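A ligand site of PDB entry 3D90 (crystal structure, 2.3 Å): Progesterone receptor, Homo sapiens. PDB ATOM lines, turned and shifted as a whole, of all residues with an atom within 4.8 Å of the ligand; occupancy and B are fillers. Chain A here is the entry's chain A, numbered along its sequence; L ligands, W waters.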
ATOM      1  N   LEU A  40      20.105 -11.294  -7.578  1.00  0.00           N
ATOM      2  CA  LEU A  40      19.210 -12.018  -6.680  1.00  0.00           C
ATOM      3  C   LEU A  40      18.480 -11.069  -5.757  1.00  0.00           C
ATOM      4  O   LEU A  40      17.289 -11.239  -5.467  1.00  0.00           O
ATOM      5  CB  LEU A  40      19.993 -13.030  -5.852  1.00  0.00           C
ATOM      6  CG  LEU A  40      20.449 -14.273  -6.612  1.00  0.00           C
ATOM      7  CD1 LEU A  40      21.203 -15.206  -5.695  1.00  0.00           C
ATOM      8  CD2 LEU A  40      19.246 -14.969  -7.201  1.00  0.00           C
ATOM      9  N   LEU A  43      15.696  -9.457  -7.501  1.00  0.00           N
ATOM     10  CA  LEU A  43      14.604 -10.392  -7.708  1.00  0.00           C
ATOM     11  C   LEU A  43      13.780 -10.577  -6.423  1.00  0.00           C
ATOM     12  O   LEU A  43      12.582 -10.837  -6.478  1.00  0.00           O
ATOM     13  CB  LEU A  43      15.127 -11.733  -8.208  1.00  0.00           C
ATOM     14  CG  LEU A  43      15.390 -11.804  -9.723  1.00  0.00           C
ATOM     15  CD1 LEU A  43      15.997 -13.158 -10.072  1.00  0.00           C
ATOM     16  CD2 LEU A  43      14.093 -11.581 -10.501  1.00  0.00           C
ATOM     17  N   ASN A  44      14.444 -10.506  -5.271  1.00  0.00           N
ATOM     18  CA  ASN A  44      13.731 -10.616  -3.996  1.00  0.00           C
ATOM     19  C   ASN A  44      12.916  -9.338  -3.757  1.00  0.00           C
ATOM     20  O   ASN A  44      11.822  -9.392  -3.170  1.00  0.00           O
ATOM     21  CB  ASN A  44      14.705 -10.817  -2.834  1.00  0.00           C
ATOM     22  CG  ASN A  44      15.467 -12.114  -2.945  1.00  0.00           C
ATOM     23  OD1 ASN A  44      15.041 -13.039  -3.639  1.00  0.00           O
ATOM     24  ND2 ASN A  44      16.596 -12.205  -2.248  1.00  0.00           N
ATOM     25  N   LEU A  46      11.597  -7.352  -6.115  1.00  0.00           N
ATOM     26  CA  LEU A  46      10.480  -7.410  -7.036  1.00  0.00           C
ATOM     27  C   LEU A  46       9.458  -8.372  -6.444  1.00  0.00           C
ATOM     28  O   LEU A  46       8.249  -8.146  -6.517  1.00  0.00           O
ATOM     29  CB  LEU A  46      10.963  -7.922  -8.397  1.00  0.00           C
ATOM     30  CG  LEU A  46      10.000  -8.004  -9.585  1.00  0.00           C
ATOM     31  CD1 LEU A  46       9.691  -6.602 -10.115  1.00  0.00           C
ATOM     32  CD2 LEU A  46      10.636  -8.855 -10.670  1.00  0.00           C
ATOM     33  N   GLY A  47       9.937  -9.463  -5.856  1.00  0.00           N
ATOM     34  CA  GLY A  47       9.056 -10.431  -5.231  1.00  0.00           C
ATOM     35  C   GLY A  47       8.325  -9.796  -4.067  1.00  0.00           C
ATOM     36  O   GLY A  47       7.118  -9.989  -3.898  1.00  0.00           O
ATOM     37  N   GLN A  50       5.692  -7.863  -5.443  1.00  0.00           N
ATOM     38  CA  GLN A  50       4.631  -8.660  -6.037  1.00  0.00           C
ATOM     39  C   GLN A  50       3.746  -9.273  -4.959  1.00  0.00           C
ATOM     40  O   GLN A  50       2.541  -9.412  -5.140  1.00  0.00           O
ATOM     41  CB  GLN A  50       5.209  -9.741  -6.958  1.00  0.00           C
ATOM     42  CG  GLN A  50       5.733  -9.163  -8.265  1.00  0.00           C
ATOM     43  CD  GLN A  50       5.978 -10.220  -9.319  1.00  0.00           C
ATOM     44  OE1 GLN A  50       5.768 -11.414  -9.083  1.00  0.00           O
ATOM     45  NE2 GLN A  50       6.435  -9.789 -10.484  1.00  0.00           N
ATOM     46  N   TRP A  80       2.125 -18.042  -3.480  1.00  0.00           N
ATOM     47  CA  TRP A  80       2.843 -16.886  -4.021  1.00  0.00           C
ATOM     48  C   TRP A  80       3.843 -17.219  -5.136  1.00  0.00           C
ATOM     49  O   TRP A  80       3.907 -16.514  -6.136  1.00  0.00           O
ATOM     50  CB  TRP A  80       3.587 -16.130  -2.924  1.00  0.00           C
ATOM     51  CG  TRP A  80       4.677 -16.909  -2.228  1.00  0.00           C
ATOM     52  CD1 TRP A  80       4.513 -17.822  -1.233  1.00  0.00           C
ATOM     53  CD2 TRP A  80       6.081 -16.818  -2.469  1.00  0.00           C
ATOM     54  NE1 TRP A  80       5.739 -18.309  -0.843  1.00  0.00           N
ATOM     55  CE2 TRP A  80       6.715 -17.710  -1.588  1.00  0.00           C
ATOM     56  CE3 TRP A  80       6.863 -16.065  -3.350  1.00  0.00           C
ATOM     57  CZ2 TRP A  80       8.099 -17.874  -1.547  1.00  0.00           C
ATOM     58  CZ3 TRP A  80       8.239 -16.226  -3.320  1.00  0.00           C
ATOM     59  CH2 TRP A  80       8.844 -17.123  -2.421  1.00  0.00           C
ATOM     60  N   MET A  81       4.615 -18.282  -4.940  1.00  0.00           N
ATOM     61  CA  MET A  81       5.643 -18.688  -5.892  1.00  0.00           C
ATOM     62  C   MET A  81       5.052 -19.066  -7.254  1.00  0.00           C
ATOM     63  O   MET A  81       5.481 -18.541  -8.280  1.00  0.00           O
ATOM     64  CB  MET A  81       6.437 -19.885  -5.334  1.00  0.00           C
ATOM     65  CG  MET A  81       7.611 -20.352  -6.185  1.00  0.00           C
ATOM     66  SD  MET A  81       9.023 -19.219  -6.177  1.00  0.00           S
ATOM     67  CE  MET A  81       9.816 -19.624  -4.622  1.00  0.00           C
ATOM     68  N   MET A  84       3.788 -16.005  -9.028  1.00  0.00           N
ATOM     69  CA  MET A  84       4.829 -15.141  -9.566  1.00  0.00           C
ATOM     70  C   MET A  84       5.517 -15.690 -10.824  1.00  0.00           C
ATOM     71  O   MET A  84       5.913 -14.930 -11.700  1.00  0.00           O
ATOM     72  CB  MET A  84       5.905 -14.846  -8.516  1.00  0.00           C
ATOM     73  CG  MET A  84       5.491 -13.907  -7.371  1.00  0.00           C
ATOM     74  SD  MET A  84       6.845 -13.651  -6.180  1.00  0.00           S
ATOM     75  CE  MET A  84       6.016 -12.587  -4.885  1.00  0.00           C
ATOM     76  N   VAL A  85       5.665 -17.012 -10.905  1.00  0.00           N
ATOM     77  CA  VAL A  85       6.306 -17.621 -12.069  1.00  0.00           C
ATOM     78  C   VAL A  85       5.306 -17.759 -13.213  1.00  0.00           C
ATOM     79  O   VAL A  85       5.676 -17.726 -14.387  1.00  0.00           O
ATOM     80  CB  VAL A  85       6.901 -19.008 -11.708  1.00  0.00           C
ATOM     81  CG1 VAL A  85       5.799 -19.949 -11.267  1.00  0.00           C
ATOM     82  CG2 VAL A  85       7.663 -19.571 -12.897  1.00  0.00           C
ATOM     83  N   LEU A  88       5.057 -14.589 -14.789  1.00  0.00           N
ATOM     84  CA  LEU A  88       6.320 -14.279 -15.433  1.00  0.00           C
ATOM     85  C   LEU A  88       6.137 -14.828 -16.839  1.00  0.00           C
ATOM     86  O   LEU A  88       6.554 -14.224 -17.815  1.00  0.00           O
ATOM     87  CB  LEU A  88       7.483 -15.005 -14.727  1.00  0.00           C
ATOM     88  CG  LEU A  88       8.825 -15.042 -15.464  1.00  0.00           C
ATOM     89  CD1 LEU A  88       9.370 -13.640 -15.655  1.00  0.00           C
ATOM     90  CD2 LEU A  88       9.802 -15.878 -14.680  1.00  0.00           C
ATOM     91  N   ARG A  91       3.836 -12.341 -18.960  1.00  0.00           N
ATOM     92  CA  ARG A  91       4.573 -11.167 -19.410  1.00  0.00           C
ATOM     93  C   ARG A  91       5.587 -11.528 -20.490  1.00  0.00           C
ATOM     94  O   ARG A  91       5.674 -10.848 -21.505  1.00  0.00           O
ATOM     95  CB  ARG A  91       5.293 -10.494 -18.224  1.00  0.00           C
ATOM     96  CG  ARG A  91       4.367  -9.712 -17.288  1.00  0.00           C
ATOM     97  CD  ARG A  91       5.166  -8.964 -16.206  1.00  0.00           C
ATOM     98  NE  ARG A  91       6.035  -9.856 -15.435  1.00  0.00           N
ATOM     99  CZ  ARG A  91       5.683 -10.461 -14.301  1.00  0.00           C
ATOM    100  NH1 ARG A  91       6.555 -11.263 -13.683  1.00  0.00           N
ATOM    101  NH2 ARG A  91       4.486 -10.256 -13.774  1.00  0.00           N
ATOM    102  N   PHE A 103      10.817 -10.339 -16.248  1.00  0.00           N
ATOM    103  CA  PHE A 103      10.449 -10.218 -14.840  1.00  0.00           C
ATOM    104  C   PHE A 103       9.747  -8.899 -14.595  1.00  0.00           C
ATOM    105  O   PHE A 103       8.677  -8.861 -13.987  1.00  0.00           O
ATOM    106  CB  PHE A 103      11.687 -10.343 -13.937  1.00  0.00           C
ATOM    107  CG  PHE A 103      12.232 -11.735 -13.862  1.00  0.00           C
ATOM    108  CD1 PHE A 103      13.293 -12.127 -14.682  1.00  0.00           C
ATOM    109  CD2 PHE A 103      11.664 -12.677 -13.020  1.00  0.00           C
ATOM    110  CE1 PHE A 103      13.772 -13.441 -14.653  1.00  0.00           C
ATOM    111  CE2 PHE A 103      12.125 -13.981 -12.984  1.00  0.00           C
ATOM    112  CZ  PHE A 103      13.186 -14.372 -13.804  1.00  0.00           C
ATOM    113  N   PHE A 119      21.672 -20.980 -11.641  1.00  0.00           N
ATOM    114  CA  PHE A 119      20.737 -19.918 -11.973  1.00  0.00           C
ATOM    115  C   PHE A 119      20.189 -20.039 -13.392  1.00  0.00           C
ATOM    116  O   PHE A 119      19.001 -19.779 -13.630  1.00  0.00           O
ATOM    117  CB  PHE A 119      21.410 -18.561 -11.815  1.00  0.00           C
ATOM    118  CG  PHE A 119      20.503 -17.398 -12.126  1.00  0.00           C
ATOM    119  CD1 PHE A 119      19.597 -16.934 -11.170  1.00  0.00           C
ATOM    120  CD2 PHE A 119      20.532 -16.783 -13.370  1.00  0.00           C
ATOM    121  CE1 PHE A 119      18.734 -15.873 -11.455  1.00  0.00           C
ATOM    122  CE2 PHE A 119      19.683 -15.720 -13.664  1.00  0.00           C
ATOM    123  CZ  PHE A 119      18.781 -15.268 -12.696  1.00  0.00           C
ATOM    124  N   LEU A 122      17.721 -22.786 -13.391  1.00  0.00           N
ATOM    125  CA  LEU A 122      16.447 -22.409 -12.801  1.00  0.00           C
ATOM    126  C   LEU A 122      15.614 -21.706 -13.869  1.00  0.00           C
ATOM    127  O   LEU A 122      14.447 -22.017 -14.076  1.00  0.00           O
ATOM    128  CB  LEU A 122      16.649 -21.462 -11.613  1.00  0.00           C
ATOM    129  CG  LEU A 122      15.395 -21.036 -10.834  1.00  0.00           C
ATOM    130  CD1 LEU A 122      14.783 -22.250 -10.136  1.00  0.00           C
ATOM    131  CD2 LEU A 122      15.747 -19.967  -9.810  1.00  0.00           C
ATOM    132  N   MET A 126      11.792 -22.242 -15.578  1.00  0.00           N
ATOM    133  CA  MET A 126      10.687 -21.289 -15.558  1.00  0.00           C
ATOM    134  C   MET A 126      10.265 -21.035 -17.001  1.00  0.00           C
ATOM    135  O   MET A 126       9.084 -20.862 -17.287  1.00  0.00           O
ATOM    136  CB  MET A 126      11.137 -19.968 -14.898  1.00  0.00           C
ATOM    137  CG  MET A 126      11.627 -20.133 -13.440  1.00  0.00           C
ATOM    138  SD  MET A 126      11.859 -18.570 -12.516  1.00  0.00           S
ATOM    139  CE  MET A 126      13.575 -18.231 -12.799  1.00  0.00           C
ATOM    140  N   LEU A 212      11.794 -24.461  -7.767  1.00  0.00           N
ATOM    141  CA  LEU A 212      11.961 -23.052  -7.417  1.00  0.00           C
ATOM    142  C   LEU A 212      12.014 -22.903  -5.893  1.00  0.00           C
ATOM    143  O   LEU A 212      12.768 -22.080  -5.370  1.00  0.00           O
ATOM    144  CB  LEU A 212      10.796 -22.222  -7.964  1.00  0.00           C
ATOM    145  CG  LEU A 212      10.773 -21.858  -9.445  1.00  0.00           C
ATOM    146  CD1 LEU A 212      10.959 -23.097 -10.311  1.00  0.00           C
ATOM    147  CD2 LEU A 212       9.444 -21.161  -9.768  1.00  0.00           C
ATOM    148  N   TYR A 215      15.468 -24.170  -4.536  1.00  0.00           N
ATOM    149  CA  TYR A 215      16.481 -23.173  -4.869  1.00  0.00           C
ATOM    150  C   TYR A 215      16.335 -21.952  -3.958  1.00  0.00           C
ATOM    151  O   TYR A 215      17.326 -21.366  -3.496  1.00  0.00           O
ATOM    152  CB  TYR A 215      16.346 -22.757  -6.337  1.00  0.00           C
ATOM    153  CG  TYR A 215      17.418 -21.806  -6.842  1.00  0.00           C
ATOM    154  CD1 TYR A 215      17.350 -20.434  -6.579  1.00  0.00           C
ATOM    155  CD2 TYR A 215      18.485 -22.276  -7.601  1.00  0.00           C
ATOM    156  CE1 TYR A 215      18.328 -19.566  -7.062  1.00  0.00           C
ATOM    157  CE2 TYR A 215      19.458 -21.416  -8.084  1.00  0.00           C
ATOM    158  CZ  TYR A 215      19.374 -20.070  -7.809  1.00  0.00           C
ATOM    159  OH  TYR A 215      20.330 -19.201  -8.294  1.00  0.00           O
ATOM    160  N   CYS A 216      15.090 -21.558  -3.721  1.00  0.00           N
ATOM    161  CA  CYS A 216      14.764 -20.415  -2.886  1.00  0.00           C
ATOM    162  C   CYS A 216      15.213 -20.616  -1.437  1.00  0.00           C
ATOM    163  O   CYS A 216      15.932 -19.781  -0.868  1.00  0.00           O
ATOM    164  CB  CYS A 216      13.248 -20.156  -2.930  1.00  0.00           C
ATOM    165  SG  CYS A 216      12.625 -18.971  -1.723  1.00  0.00           S
ATOM    166  N   THR A 219      18.979 -20.593  -1.087  1.00  0.00           N
ATOM    167  CA  THR A 219      19.502 -19.247  -1.264  1.00  0.00           C
ATOM    168  C   THR A 219      19.206 -18.399  -0.017  1.00  0.00           C
ATOM    169  O   THR A 219      19.971 -17.512   0.358  1.00  0.00           O
ATOM    170  CB  THR A 219      18.859 -18.581  -2.503  1.00  0.00           C
ATOM    171  OG1 THR A 219      19.199 -19.344  -3.665  1.00  0.00           O
ATOM    172  CG2 THR A 219      19.326 -17.146  -2.665  1.00  0.00           C
ATOM    173  N   PHE A 230      16.971 -10.492   1.704  1.00  0.00           N
ATOM    174  CA  PHE A 230      15.556 -10.877   1.575  1.00  0.00           C
ATOM    175  C   PHE A 230      14.706  -9.906   2.384  1.00  0.00           C
ATOM    176  O   PHE A 230      14.993  -9.659   3.553  1.00  0.00           O
ATOM    177  CB  PHE A 230      15.306 -12.291   2.118  1.00  0.00           C
ATOM    178  CG  PHE A 230      15.713 -13.393   1.195  1.00  0.00           C
ATOM    179  CD1 PHE A 230      17.048 -13.759   1.074  1.00  0.00           C
ATOM    180  CD2 PHE A 230      14.762 -14.056   0.432  1.00  0.00           C
ATOM    181  CE1 PHE A 230      17.420 -14.781   0.208  1.00  0.00           C
ATOM    182  CE2 PHE A 230      15.125 -15.074  -0.434  1.00  0.00           C
ATOM    183  CZ  PHE A 230      16.460 -15.440  -0.555  1.00  0.00           C
ATOM    184  N   ILE A 238       8.302 -17.352   3.302  1.00  0.00           N
ATOM    185  CA  ILE A 238       9.346 -18.341   3.109  1.00  0.00           C
ATOM    186  C   ILE A 238       9.498 -19.192   4.357  1.00  0.00           C
ATOM    187  O   ILE A 238       9.283 -20.402   4.343  1.00  0.00           O
ATOM    188  CB  ILE A 238      10.708 -17.672   2.785  1.00  0.00           C
ATOM    189  CG1 ILE A 238      10.703 -17.108   1.361  1.00  0.00           C
ATOM    190  CG2 ILE A 238      11.836 -18.682   2.945  1.00  0.00           C
ATOM    191  CD1 ILE A 238      11.976 -16.374   0.951  1.00  0.00           C
HETATM  192  C1  LIG L   1      10.446 -12.248  -8.731  1.00  0.00           C
HETATM  193  C2  LIG L   1       9.192 -11.555  -9.330  1.00  0.00           C
HETATM  194  C3  LIG L   1       8.692 -12.416 -10.665  1.00  0.00           C
HETATM  195  C4  LIG L   1       8.746 -13.870 -10.748  1.00  0.00           C
HETATM  196  C5  LIG L   1       9.413 -14.537  -9.669  1.00  0.00           C
HETATM  197  C6  LIG L   1       9.346 -16.131  -9.756  1.00  0.00           C
HETATM  198  C7  LIG L   1      10.522 -16.961  -9.279  1.00  0.00           C
HETATM  199  C8  LIG L   1      11.299 -16.348  -8.000  1.00  0.00           C
HETATM  200  C9  LIG L   1      11.441 -14.666  -8.018  1.00  0.00           C
HETATM  201  C10 LIG L   1      10.235 -13.863  -8.474  1.00  0.00           C
HETATM  202  C11 LIG L   1      12.372 -13.991  -6.935  1.00  0.00           C
HETATM  203  C12 LIG L   1      13.518 -14.841  -6.479  1.00  0.00           C
HETATM  204  C13 LIG L   1      13.291 -16.512  -6.166  1.00  0.00           C
HETATM  205  C14 LIG L   1      12.542 -17.165  -7.468  1.00  0.00           C
HETATM  206  C15 LIG L   1      12.706 -18.724  -7.367  1.00  0.00           C
HETATM  207  C16 LIG L   1      13.970 -18.964  -6.438  1.00  0.00           C
HETATM  208  C17 LIG L   1      14.594 -17.483  -6.045  1.00  0.00           C
HETATM  209  C18 LIG L   1      12.275 -16.650  -4.884  1.00  0.00           C
HETATM  210  C19 LIG L   1      12.706 -15.799  -3.584  1.00  0.00           C
HETATM  211  C20 LIG L   1      15.701 -16.891  -6.989  1.00  0.00           C
HETATM  212  C21 LIG L   1      16.635 -16.231  -7.997  1.00  0.00           C
HETATM  213  O1  LIG L   1       8.158 -11.895 -11.635  1.00  0.00           O
HETATM  214  O2  LIG L   1      15.252 -17.488  -4.894  1.00  0.00           O
HETATM  215  O   HOH W   1      12.098 -13.390  -1.309  1.00  0.00           O
HETATM  216  O   HOH W   2       5.063 -12.468 -11.485  1.00  0.00           O
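The guanidinium group (NH1) of Arg 91 sits at hydrogen-bond distance from an oxygen (O1) of the ligand (2.7 Å). The side-chain amide nitrogen (NE2) of Gln 50 lies within hydrogen-bond range of an oxygen (O1) of the ligand (3.0 Å).
The guanidinium group (NE) of Arg 91 is in hydrogen-bond range of the backbone carbonyl oxygen (O) of Phe 103, at 3.2 Å. The backbone carbonyl oxygen (O) of Leu 40 lies close to the side-chain amide oxygen (OD1) of Asn 44, at 3.4 Å. The side-chain hydroxyl (OG1) of Thr 219 is in hydrogen-bond range of the backbone carbonyl oxygen (O) of Tyr 215, at 2.8 Å.
Leu 40 touches the ligand. Leu 43 touches the ligand (O to C11, 3.2 Å). Asn 44 touches the ligand. Leu 46 touches the ligand (CD2 to C2, 3.3 Å). CE of Met 81 touches C18 of the ligand, 3.9 Å away. Met 84 touches the ligand (O to C4, 3.2 Å). Val 85 touches the ligand. CD2 of Phe 103 touches C3 of the ligand (3.8 Å). Leu 122 touches the ligand. Met 126 touches the ligand (SD to C7, 3.9 Å). Leu 212 touches the ligand. Tyr 215 touches the ligand. CA of Cys 216 touches O2 of the ligand, at 3.6 Å. The nearest printed residue that does not touch the ligand is Gly 47 (4.03 Å).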
